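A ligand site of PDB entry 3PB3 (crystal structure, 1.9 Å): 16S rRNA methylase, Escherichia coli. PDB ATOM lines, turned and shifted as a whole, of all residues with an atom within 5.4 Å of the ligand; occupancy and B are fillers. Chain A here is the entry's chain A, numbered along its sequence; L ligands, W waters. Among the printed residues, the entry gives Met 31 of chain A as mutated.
OD1 of Asp 55 sits at hydrogen-bond distance from N of Thr 33 (3.4 Å). OG1 of Thr 33 is in hydrogen-bond range of OD2 of Asp 30, 2.7 Å away. N of Gly 34 lies within hydrogen-bond range of OD1 of Asp 55 (2.8 Å). The backbone NH (N) of Ala 85 is in hydrogen-bond range of the backbone carbonyl oxygen (O) of Asp 55 (3.4 Å). N of Ala 198 is in hydrogen-bond range of OG of Ser 195, 3.0 Å away. N of Gly 32 lies within hydrogen-bond range of O of Ile 54, 2.8 Å away. The backbone carbonyl oxygen of Phe 105 is in hydrogen-bond range of the indole nitrogen of Trp 197 (2.9 Å). N of Thr 33 is in hydrogen-bond range of O of Ile 54 (2.8 Å).
Met 31 touches the ligand (SD to C13, 3.9 Å). Thr 33 touches the ligand. Gly 34 touches the ligand. CD of Pro 56 touches N6 of the ligand, at 3.2 Å. CG2 of Val 57 touches O5 of the ligand, at 3.5 Å. Ala 86 touches the ligand. Phe 105 touches the ligand (CD2 to O2, 3.3 Å). Trp 107 touches the ligand. Tyr 113 touches the ligand (CE2 to N4, 3.5 Å). Trp 197 touches the ligand. 19 residues have an atom within 4 Å of the ligand: Met 31, Gly 32, Thr 33, Gly 34, Asn 38, Asp 55, Pro 56, Val 57, Ala 86, Ala 87, Glu 88, Leu 104, Phe 105, Trp 107, Thr 109, Leu 110, Tyr 113, Ser 195 and Trp 197.
Water W3 lies within hydrogen-bond range of the side-chain carboxylate (OD2) of Asp 30 (2.7 Å), a nitrogen (N1) of the ligand (2.8 Å), the backbone carbonyl oxygen (O) of Thr 33 (2.8 Å) and the side-chain amide nitrogen (ND2) of Asn 38 (3.0 Å). Water W6 bridges the backbone NH of Asp 35 (2.8 Å) and an oxygen (O1) of the ligand (2.9 Å). Water W5 lies within hydrogen-bond range of the backbone carbonyl oxygen of Gly 32 (3.0 Å), the backbone carbonyl oxygen of Leu 104 (3.0 Å) and a nitrogen (N1) of the ligand (3.4 Å).
The side-chain hydroxyl (OG) of Ser 195 lies within hydrogen-bond range of an oxygen (O1) of the ligand (2.6 Å). A nitrogen (N1) of the ligand is in hydrogen-bond range of the backbone carbonyl oxygen of Gly 32 (2.8 Å). The backbone NH of Ala 87 sits at hydrogen-bond distance from a nitrogen (N5) of the ligand. N of Leu 110 sits at hydrogen-bond distance from N3 of the ligand (3.4 Å). O5 of the ligand lies within hydrogen-bond range of OD2 of Asp 55, at 2.6 Å. A nitrogen (N1) of the ligand is in hydrogen-bond range of the backbone carbonyl oxygen (O) of Leu 104, at 2.7 Å. The side-chain amide nitrogen (ND2) of Asn 38 is in hydrogen-bond range of an oxygen (O2) of the ligand (2.9 Å). N3 of the ligand lies within hydrogen-bond range of OG1 of Thr 109. A nitrogen (N4) of the ligand is in hydrogen-bond range of the side-chain carboxylate (OE1) of Glu 88, at 3.0 Å.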
ATOM      1  N   ASP A  30      -2.189  20.180 -25.890  1.00  0.00           N
ATOM      2  CA  ASP A  30      -1.950  21.617 -25.785  1.00  0.00           C
ATOM      3  C   ASP A  30      -1.737  21.931 -24.300  1.00  0.00           C
ATOM      4  O   ASP A  30      -2.678  21.861 -23.510  1.00  0.00           O
ATOM      5  CB  ASP A  30      -3.159  22.378 -26.355  1.00  0.00           C
ATOM      6  CG  ASP A  30      -2.913  23.884 -26.475  1.00  0.00           C
ATOM      7  OD1 ASP A  30      -1.797  24.313 -26.844  1.00  0.00           O
ATOM      8  OD2 ASP A  30      -3.870  24.653 -26.194  1.00  0.00           O
ATOM      9  N   MET A  31      -0.497  22.264 -23.938  1.00  0.00           N
ATOM     10  CA  MET A  31      -0.136  22.560 -22.541  1.00  0.00           C
ATOM     11  C   MET A  31      -0.337  24.053 -22.254  1.00  0.00           C
ATOM     12  O   MET A  31       0.101  24.889 -23.029  1.00  0.00           O
ATOM     13  CB  MET A  31       1.317  22.140 -22.274  1.00  0.00           C
ATOM     14  CG  MET A  31       1.872  22.550 -20.891  1.00  0.00           C
ATOM     15  SD  MET A  31       0.970  21.772 -19.520  1.00  0.00           S
ATOM     16  CE  MET A  31       1.695  20.148 -19.543  1.00  0.00           C
ATOM     17  N   GLY A  32      -0.956  24.378 -21.122  1.00  0.00           N
ATOM     18  CA  GLY A  32      -1.318  25.762 -20.797  1.00  0.00           C
ATOM     19  C   GLY A  32      -2.372  26.245 -21.782  1.00  0.00           C
ATOM     20  O   GLY A  32      -2.236  27.331 -22.365  1.00  0.00           O
ATOM     21  N   THR A  33      -3.408  25.436 -21.952  1.00  0.00           N
ATOM     22  CA  THR A  33      -4.417  25.633 -23.000  1.00  0.00           C
ATOM     23  C   THR A  33      -5.264  26.899 -22.835  1.00  0.00           C
ATOM     24  O   THR A  33      -5.803  27.417 -23.809  1.00  0.00           O
ATOM     25  CB  THR A  33      -5.312  24.375 -23.183  1.00  0.00           C
ATOM     26  OG1 THR A  33      -5.883  24.358 -24.495  1.00  0.00           O
ATOM     27  CG2 THR A  33      -6.427  24.312 -22.126  1.00  0.00           C
ATOM     28  N   GLY A  34      -5.374  27.397 -21.604  1.00  0.00           N
ATOM     29  CA  GLY A  34      -6.105  28.641 -21.368  1.00  0.00           C
ATOM     30  C   GLY A  34      -7.604  28.406 -21.431  1.00  0.00           C
ATOM     31  O   GLY A  34      -8.106  27.496 -20.774  1.00  0.00           O
ATOM     32  N   ASP A  35      -8.311  29.214 -22.224  1.00  0.00           N
ATOM     33  CA  ASP A  35      -9.787  29.190 -22.247  1.00  0.00           C
ATOM     34  C   ASP A  35     -10.412  28.060 -23.063  1.00  0.00           C
ATOM     35  O   ASP A  35     -11.630  27.922 -23.103  1.00  0.00           O
ATOM     36  CB  ASP A  35     -10.356  30.561 -22.656  1.00  0.00           C
ATOM     37  CG  ASP A  35     -10.034  30.959 -24.090  1.00  0.00           C
ATOM     38  OD1 ASP A  35      -9.696  30.081 -24.920  1.00  0.00           O
ATOM     39  OD2 ASP A  35     -10.112  32.174 -24.395  1.00  0.00           O
ATOM     40  N   ASN A  38      -8.784  27.751 -28.455  1.00  0.00           N
ATOM     41  CA  ASN A  38      -7.825  27.324 -29.471  1.00  0.00           C
ATOM     42  C   ASN A  38      -7.980  25.848 -29.784  1.00  0.00           C
ATOM     43  O   ASN A  38      -7.996  25.453 -30.964  1.00  0.00           O
ATOM     44  CB  ASN A  38      -6.381  27.588 -29.015  1.00  0.00           C
ATOM     45  CG  ASN A  38      -6.020  29.051 -29.005  1.00  0.00           C
ATOM     46  OD1 ASN A  38      -6.663  29.877 -29.667  1.00  0.00           O
ATOM     47  ND2 ASN A  38      -4.984  29.389 -28.238  1.00  0.00           N
ATOM     48  N   ILE A  54      -4.519  21.061 -21.443  1.00  0.00           N
ATOM     49  CA  ILE A  54      -4.115  21.017 -20.045  1.00  0.00           C
ATOM     50  C   ILE A  54      -3.933  22.431 -19.493  1.00  0.00           C
ATOM     51  O   ILE A  54      -3.270  23.265 -20.112  1.00  0.00           O
ATOM     52  CB  ILE A  54      -2.791  20.247 -19.849  1.00  0.00           C
ATOM     53  CG1 ILE A  54      -2.821  18.894 -20.579  1.00  0.00           C
ATOM     54  CG2 ILE A  54      -2.487  20.040 -18.362  1.00  0.00           C
ATOM     55  CD1 ILE A  54      -1.479  18.170 -20.568  1.00  0.00           C
ATOM     56  N   ASP A  55      -4.536  22.691 -18.328  1.00  0.00           N
ATOM     57  CA  ASP A  55      -4.376  23.983 -17.653  1.00  0.00           C
ATOM     58  C   ASP A  55      -4.733  23.838 -16.169  1.00  0.00           C
ATOM     59  O   ASP A  55      -5.686  23.159 -15.825  1.00  0.00           O
ATOM     60  CB  ASP A  55      -5.268  25.061 -18.299  1.00  0.00           C
ATOM     61  CG  ASP A  55      -4.703  26.464 -18.123  1.00  0.00           C
ATOM     62  OD1 ASP A  55      -4.212  27.037 -19.120  1.00  0.00           O
ATOM     63  OD2 ASP A  55      -4.741  26.995 -16.992  1.00  0.00           O
ATOM     64  N   PRO A  56      -3.945  24.474 -15.279  1.00  0.00           N
ATOM     65  CA  PRO A  56      -4.268  24.412 -13.851  1.00  0.00           C
ATOM     66  C   PRO A  56      -5.460  25.288 -13.440  1.00  0.00           C
ATOM     67  O   PRO A  56      -5.933  25.180 -12.299  1.00  0.00           O
ATOM     68  CB  PRO A  56      -2.988  24.902 -13.169  1.00  0.00           C
ATOM     69  CG  PRO A  56      -2.323  25.785 -14.208  1.00  0.00           C
ATOM     70  CD  PRO A  56      -2.641  25.136 -15.525  1.00  0.00           C
ATOM     71  N   VAL A  57      -5.940  26.139 -14.344  1.00  0.00           N
ATOM     72  CA  VAL A  57      -7.079  27.025 -14.038  1.00  0.00           C
ATOM     73  C   VAL A  57      -8.373  26.484 -14.646  1.00  0.00           C
ATOM     74  O   VAL A  57      -8.683  26.756 -15.811  1.00  0.00           O
ATOM     75  CB  VAL A  57      -6.796  28.491 -14.503  1.00  0.00           C
ATOM     76  CG1 VAL A  57      -7.997  29.410 -14.199  1.00  0.00           C
ATOM     77  CG2 VAL A  57      -5.525  29.033 -13.856  1.00  0.00           C
ATOM     78  N   ALA A  85      -4.336  20.272 -14.617  1.00  0.00           N
ATOM     79  CA  ALA A  85      -3.020  19.954 -14.089  1.00  0.00           C
ATOM     80  C   ALA A  85      -2.042  21.021 -14.541  1.00  0.00           C
ATOM     81  O   ALA A  85      -2.362  21.820 -15.425  1.00  0.00           O
ATOM     82  CB  ALA A  85      -2.575  18.566 -14.568  1.00  0.00           C
ATOM     83  N   ALA A  86      -0.852  21.031 -13.953  1.00  0.00           N
ATOM     84  CA  ALA A  86       0.190  21.967 -14.345  1.00  0.00           C
ATOM     85  C   ALA A  86       1.350  21.247 -15.033  1.00  0.00           C
ATOM     86  O   ALA A  86       1.449  20.021 -14.960  1.00  0.00           O
ATOM     87  CB  ALA A  86       0.682  22.751 -13.122  1.00  0.00           C
ATOM     88  N   ALA A  87       2.216  22.014 -15.699  1.00  0.00           N
ATOM     89  CA  ALA A  87       3.428  21.468 -16.318  1.00  0.00           C
ATOM     90  C   ALA A  87       4.309  20.701 -15.318  1.00  0.00           C
ATOM     91  O   ALA A  87       5.015  19.762 -15.700  1.00  0.00           O
ATOM     92  CB  ALA A  87       4.223  22.584 -16.977  1.00  0.00           C
ATOM     93  N   GLU A  88       4.258  21.105 -14.043  1.00  0.00           N
ATOM     94  CA  GLU A  88       4.979  20.436 -12.956  1.00  0.00           C
ATOM     95  C   GLU A  88       4.402  19.060 -12.572  1.00  0.00           C
ATOM     96  O   GLU A  88       5.093  18.237 -11.966  1.00  0.00           O
ATOM     97  CB  GLU A  88       4.998  21.335 -11.699  1.00  0.00           C
ATOM     98  CG  GLU A  88       5.686  22.704 -11.839  1.00  0.00           C
ATOM     99  CD  GLU A  88       4.746  23.828 -12.281  1.00  0.00           C
ATOM    100  OE1 GLU A  88       3.788  23.555 -13.031  1.00  0.00           O
ATOM    101  OE2 GLU A  88       4.973  24.994 -11.889  1.00  0.00           O
ATOM    102  N   LEU A 104       1.276  27.370 -26.601  1.00  0.00           N
ATOM    103  CA  LEU A 104       0.955  28.580 -27.360  1.00  0.00           C
ATOM    104  C   LEU A 104       0.766  29.803 -26.468  1.00  0.00           C
ATOM    105  O   LEU A 104      -0.032  29.764 -25.536  1.00  0.00           O
ATOM    106  CB  LEU A 104      -0.311  28.358 -28.187  1.00  0.00           C
ATOM    107  CG  LEU A 104      -0.350  27.125 -29.094  1.00  0.00           C
ATOM    108  CD1 LEU A 104      -1.754  26.950 -29.647  1.00  0.00           C
ATOM    109  CD2 LEU A 104       0.676  27.253 -30.213  1.00  0.00           C
ATOM    110  N   PHE A 105       1.500  30.870 -26.775  1.00  0.00           N
ATOM    111  CA  PHE A 105       1.377  32.154 -26.071  1.00  0.00           C
ATOM    112  C   PHE A 105       1.378  32.000 -24.549  1.00  0.00           C
ATOM    113  O   PHE A 105       0.514  32.568 -23.869  1.00  0.00           O
ATOM    114  CB  PHE A 105       0.121  32.887 -26.569  1.00  0.00           C
ATOM    115  CG  PHE A 105      -0.062  32.822 -28.058  1.00  0.00           C
ATOM    116  CD1 PHE A 105       0.767  33.548 -28.907  1.00  0.00           C
ATOM    117  CD2 PHE A 105      -1.044  32.007 -28.618  1.00  0.00           C
ATOM    118  CE1 PHE A 105       0.610  33.479 -30.302  1.00  0.00           C
ATOM    119  CE2 PHE A 105      -1.207  31.927 -29.996  1.00  0.00           C
ATOM    120  CZ  PHE A 105      -0.374  32.661 -30.843  1.00  0.00           C
ATOM    121  N   PRO A 106       2.350  31.233 -23.996  1.00  0.00           N
ATOM    122  CA  PRO A 106       2.353  31.015 -22.553  1.00  0.00           C
ATOM    123  C   PRO A 106       2.619  32.318 -21.784  1.00  0.00           C
ATOM    124  O   PRO A 106       3.166  33.279 -22.328  1.00  0.00           O
ATOM    125  CB  PRO A 106       3.515  30.044 -22.351  1.00  0.00           C
ATOM    126  CG  PRO A 106       4.446  30.347 -23.467  1.00  0.00           C
ATOM    127  CD  PRO A 106       3.546  30.642 -24.633  1.00  0.00           C
ATOM    128  N   TRP A 107       2.196  32.332 -20.520  1.00  0.00           N
ATOM    129  CA  TRP A 107       2.391  33.493 -19.655  1.00  0.00           C
ATOM    130  C   TRP A 107       2.713  32.950 -18.261  1.00  0.00           C
ATOM    131  O   TRP A 107       2.553  31.747 -18.011  1.00  0.00           O
ATOM    132  CB  TRP A 107       1.122  34.358 -19.640  1.00  0.00           C
ATOM    133  CG  TRP A 107       1.360  35.834 -19.439  1.00  0.00           C
ATOM    134  CD1 TRP A 107       2.031  36.681 -20.279  1.00  0.00           C
ATOM    135  CD2 TRP A 107       0.896  36.648 -18.348  1.00  0.00           C
ATOM    136  NE1 TRP A 107       2.024  37.957 -19.777  1.00  0.00           N
ATOM    137  CE2 TRP A 107       1.335  37.964 -18.593  1.00  0.00           C
ATOM    138  CE3 TRP A 107       0.151  36.390 -17.195  1.00  0.00           C
ATOM    139  CZ2 TRP A 107       1.055  39.030 -17.722  1.00  0.00           C
ATOM    140  CZ3 TRP A 107      -0.126  37.433 -16.327  1.00  0.00           C
ATOM    141  CH2 TRP A 107       0.334  38.745 -16.591  1.00  0.00           C
ATOM    142  N   GLY A 108       3.180  33.813 -17.376  1.00  0.00           N
ATOM    143  CA  GLY A 108       3.516  33.388 -16.005  1.00  0.00           C
ATOM    144  C   GLY A 108       4.638  32.372 -15.955  1.00  0.00           C
ATOM    145  O   GLY A 108       5.578  32.435 -16.767  1.00  0.00           O
ATOM    146  N   THR A 109       4.528  31.404 -15.050  1.00  0.00           N
ATOM    147  CA  THR A 109       5.575  30.381 -14.867  1.00  0.00           C
ATOM    148  C   THR A 109       5.854  29.590 -16.138  1.00  0.00           C
ATOM    149  O   THR A 109       7.000  29.286 -16.448  1.00  0.00           O
ATOM    150  CB  THR A 109       5.263  29.401 -13.711  1.00  0.00           C
ATOM    151  OG1 THR A 109       3.959  28.814 -13.901  1.00  0.00           O
ATOM    152  CG2 THR A 109       5.305  30.117 -12.375  1.00  0.00           C
ATOM    153  N   LEU A 110       4.806  29.251 -16.876  1.00  0.00           N
ATOM    154  CA  LEU A 110       4.956  28.443 -18.082  1.00  0.00           C
ATOM    155  C   LEU A 110       5.830  29.142 -19.122  1.00  0.00           C
ATOM    156  O   LEU A 110       6.620  28.492 -19.801  1.00  0.00           O
ATOM    157  CB  LEU A 110       3.591  28.079 -18.685  1.00  0.00           C
ATOM    158  CG  LEU A 110       3.628  27.090 -19.857  1.00  0.00           C
ATOM    159  CD1 LEU A 110       4.347  25.797 -19.472  1.00  0.00           C
ATOM    160  CD2 LEU A 110       2.230  26.802 -20.332  1.00  0.00           C
ATOM    161  N   TYR A 113       9.483  28.740 -18.095  1.00  0.00           N
ATOM    162  CA  TYR A 113       9.897  27.340 -18.315  1.00  0.00           C
ATOM    163  C   TYR A 113      10.320  27.099 -19.762  1.00  0.00           C
ATOM    164  O   TYR A 113      11.264  26.354 -20.030  1.00  0.00           O
ATOM    165  CB  TYR A 113       8.791  26.345 -17.939  1.00  0.00           C
ATOM    166  CG  TYR A 113       8.393  26.346 -16.470  1.00  0.00           C
ATOM    167  CD1 TYR A 113       9.310  26.689 -15.472  1.00  0.00           C
ATOM    168  CD2 TYR A 113       7.099  25.990 -16.081  1.00  0.00           C
ATOM    169  CE1 TYR A 113       8.950  26.687 -14.122  1.00  0.00           C
ATOM    170  CE2 TYR A 113       6.723  25.972 -14.734  1.00  0.00           C
ATOM    171  CZ  TYR A 113       7.656  26.325 -13.764  1.00  0.00           C
ATOM    172  OH  TYR A 113       7.295  26.316 -12.435  1.00  0.00           O
ATOM    173  N   SER A 195      -8.655  31.962 -28.981  1.00  0.00           N
ATOM    174  CA  SER A 195      -8.650  32.342 -27.561  1.00  0.00           C
ATOM    175  C   SER A 195      -8.683  33.860 -27.405  1.00  0.00           C
ATOM    176  O   SER A 195      -8.176  34.585 -28.248  1.00  0.00           O
ATOM    177  CB  SER A 195      -7.454  31.741 -26.819  1.00  0.00           C
ATOM    178  OG  SER A 195      -6.296  32.544 -26.942  1.00  0.00           O
ATOM    179  N   TRP A 197      -7.174  35.639 -25.229  1.00  0.00           N
ATOM    180  CA  TRP A 197      -5.785  36.031 -25.026  1.00  0.00           C
ATOM    181  C   TRP A 197      -5.055  36.248 -26.348  1.00  0.00           C
ATOM    182  O   TRP A 197      -4.408  37.275 -26.547  1.00  0.00           O
ATOM    183  CB  TRP A 197      -5.088  34.949 -24.189  1.00  0.00           C
ATOM    184  CG  TRP A 197      -3.602  35.118 -23.963  1.00  0.00           C
ATOM    185  CD1 TRP A 197      -2.627  34.220 -24.289  1.00  0.00           C
ATOM    186  CD2 TRP A 197      -2.927  36.231 -23.347  1.00  0.00           C
ATOM    187  NE1 TRP A 197      -1.397  34.696 -23.919  1.00  0.00           N
ATOM    188  CE2 TRP A 197      -1.545  35.923 -23.327  1.00  0.00           C
ATOM    189  CE3 TRP A 197      -3.355  37.450 -22.797  1.00  0.00           C
ATOM    190  CZ2 TRP A 197      -0.593  36.797 -22.793  1.00  0.00           C
ATOM    191  CZ3 TRP A 197      -2.401  38.325 -22.272  1.00  0.00           C
ATOM    192  CH2 TRP A 197      -1.032  37.981 -22.269  1.00  0.00           C
ATOM    193  N   ALA A 198      -5.151  35.262 -27.249  1.00  0.00           N
ATOM    194  CA  ALA A 198      -4.508  35.393 -28.572  1.00  0.00           C
ATOM    195  C   ALA A 198      -5.047  36.591 -29.355  1.00  0.00           C
ATOM    196  O   ALA A 198      -4.280  37.295 -30.010  1.00  0.00           O
ATOM    197  CB  ALA A 198      -4.682  34.105 -29.369  1.00  0.00           C
HETATM  198  N1  LIG L   1      -2.393  28.779 -24.727  1.00  0.00           N
HETATM  199  C1  LIG L   1      -3.250  29.879 -24.199  1.00  0.00           C
HETATM  200  C2  LIG L   1      -2.451  30.755 -23.225  1.00  0.00           C
HETATM  201  C3  LIG L   1      -3.367  31.386 -22.167  1.00  0.00           C
HETATM  202  S1  LIG L   1      -2.491  32.408 -21.013  1.00  0.00           S
HETATM  203  C4  LIG L   1      -3.777  30.711 -25.334  1.00  0.00           C
HETATM  204  O1  LIG L   1      -4.816  31.333 -25.153  1.00  0.00           O
HETATM  205  O2  LIG L   1      -3.232  30.787 -26.442  1.00  0.00           O
HETATM  206  C5  LIG L   1      -1.323  31.346 -20.234  1.00  0.00           C
HETATM  207  C6  LIG L   1      -1.957  30.075 -19.649  1.00  0.00           C
HETATM  208  O3  LIG L   1      -0.895  29.219 -19.209  1.00  0.00           O
HETATM  209  C7  LIG L   1      -2.875  30.303 -18.441  1.00  0.00           C
HETATM  210  O4  LIG L   1      -4.153  29.718 -18.699  1.00  0.00           O
HETATM  211  C8  LIG L   1      -2.179  29.579 -17.294  1.00  0.00           C
HETATM  212  O5  LIG L   1      -3.077  28.939 -16.360  1.00  0.00           O
HETATM  213  C9  LIG L   1      -1.287  28.572 -17.998  1.00  0.00           C
HETATM  214  N2  LIG L   1      -0.116  28.232 -17.154  1.00  0.00           N
HETATM  215  C10 LIG L   1       0.676  29.099 -16.486  1.00  0.00           C
HETATM  216  N3  LIG L   1       1.639  28.442 -15.798  1.00  0.00           N
HETATM  217  C11 LIG L   1       1.465  27.130 -16.020  1.00  0.00           C
HETATM  218  C12 LIG L   1       2.144  25.879 -15.603  1.00  0.00           C
HETATM  219  N4  LIG L   1       3.222  25.912 -14.781  1.00  0.00           N
HETATM  220  N5  LIG L   1       1.642  24.708 -16.066  1.00  0.00           N
HETATM  221  C13 LIG L   1       0.571  24.662 -16.890  1.00  0.00           C
HETATM  222  N6  LIG L   1      -0.083  25.753 -17.315  1.00  0.00           N
HETATM  223  C14 LIG L   1       0.311  26.997 -16.915  1.00  0.00           C
HETATM  224  O   HOH W   1      -6.750  30.446 -18.116  1.00  0.00           O
HETATM  225  O   HOH W   2      -1.752  29.419 -13.960  1.00  0.00           O
HETATM  226  O   HOH W   3      -4.290  27.332 -26.181  1.00  0.00           O
HETATM  227  O   HOH W   4      -0.361  31.842 -14.706  1.00  0.00           O
HETATM  228  O   HOH W   5       0.482  28.404 -22.879  1.00  0.00           O
HETATM  229  O   HOH W   6      -6.906  31.482 -23.110  1.00  0.00           O
HETATM  230  O   HOH W   7      -0.850  26.315 -25.137  1.00  0.00           O
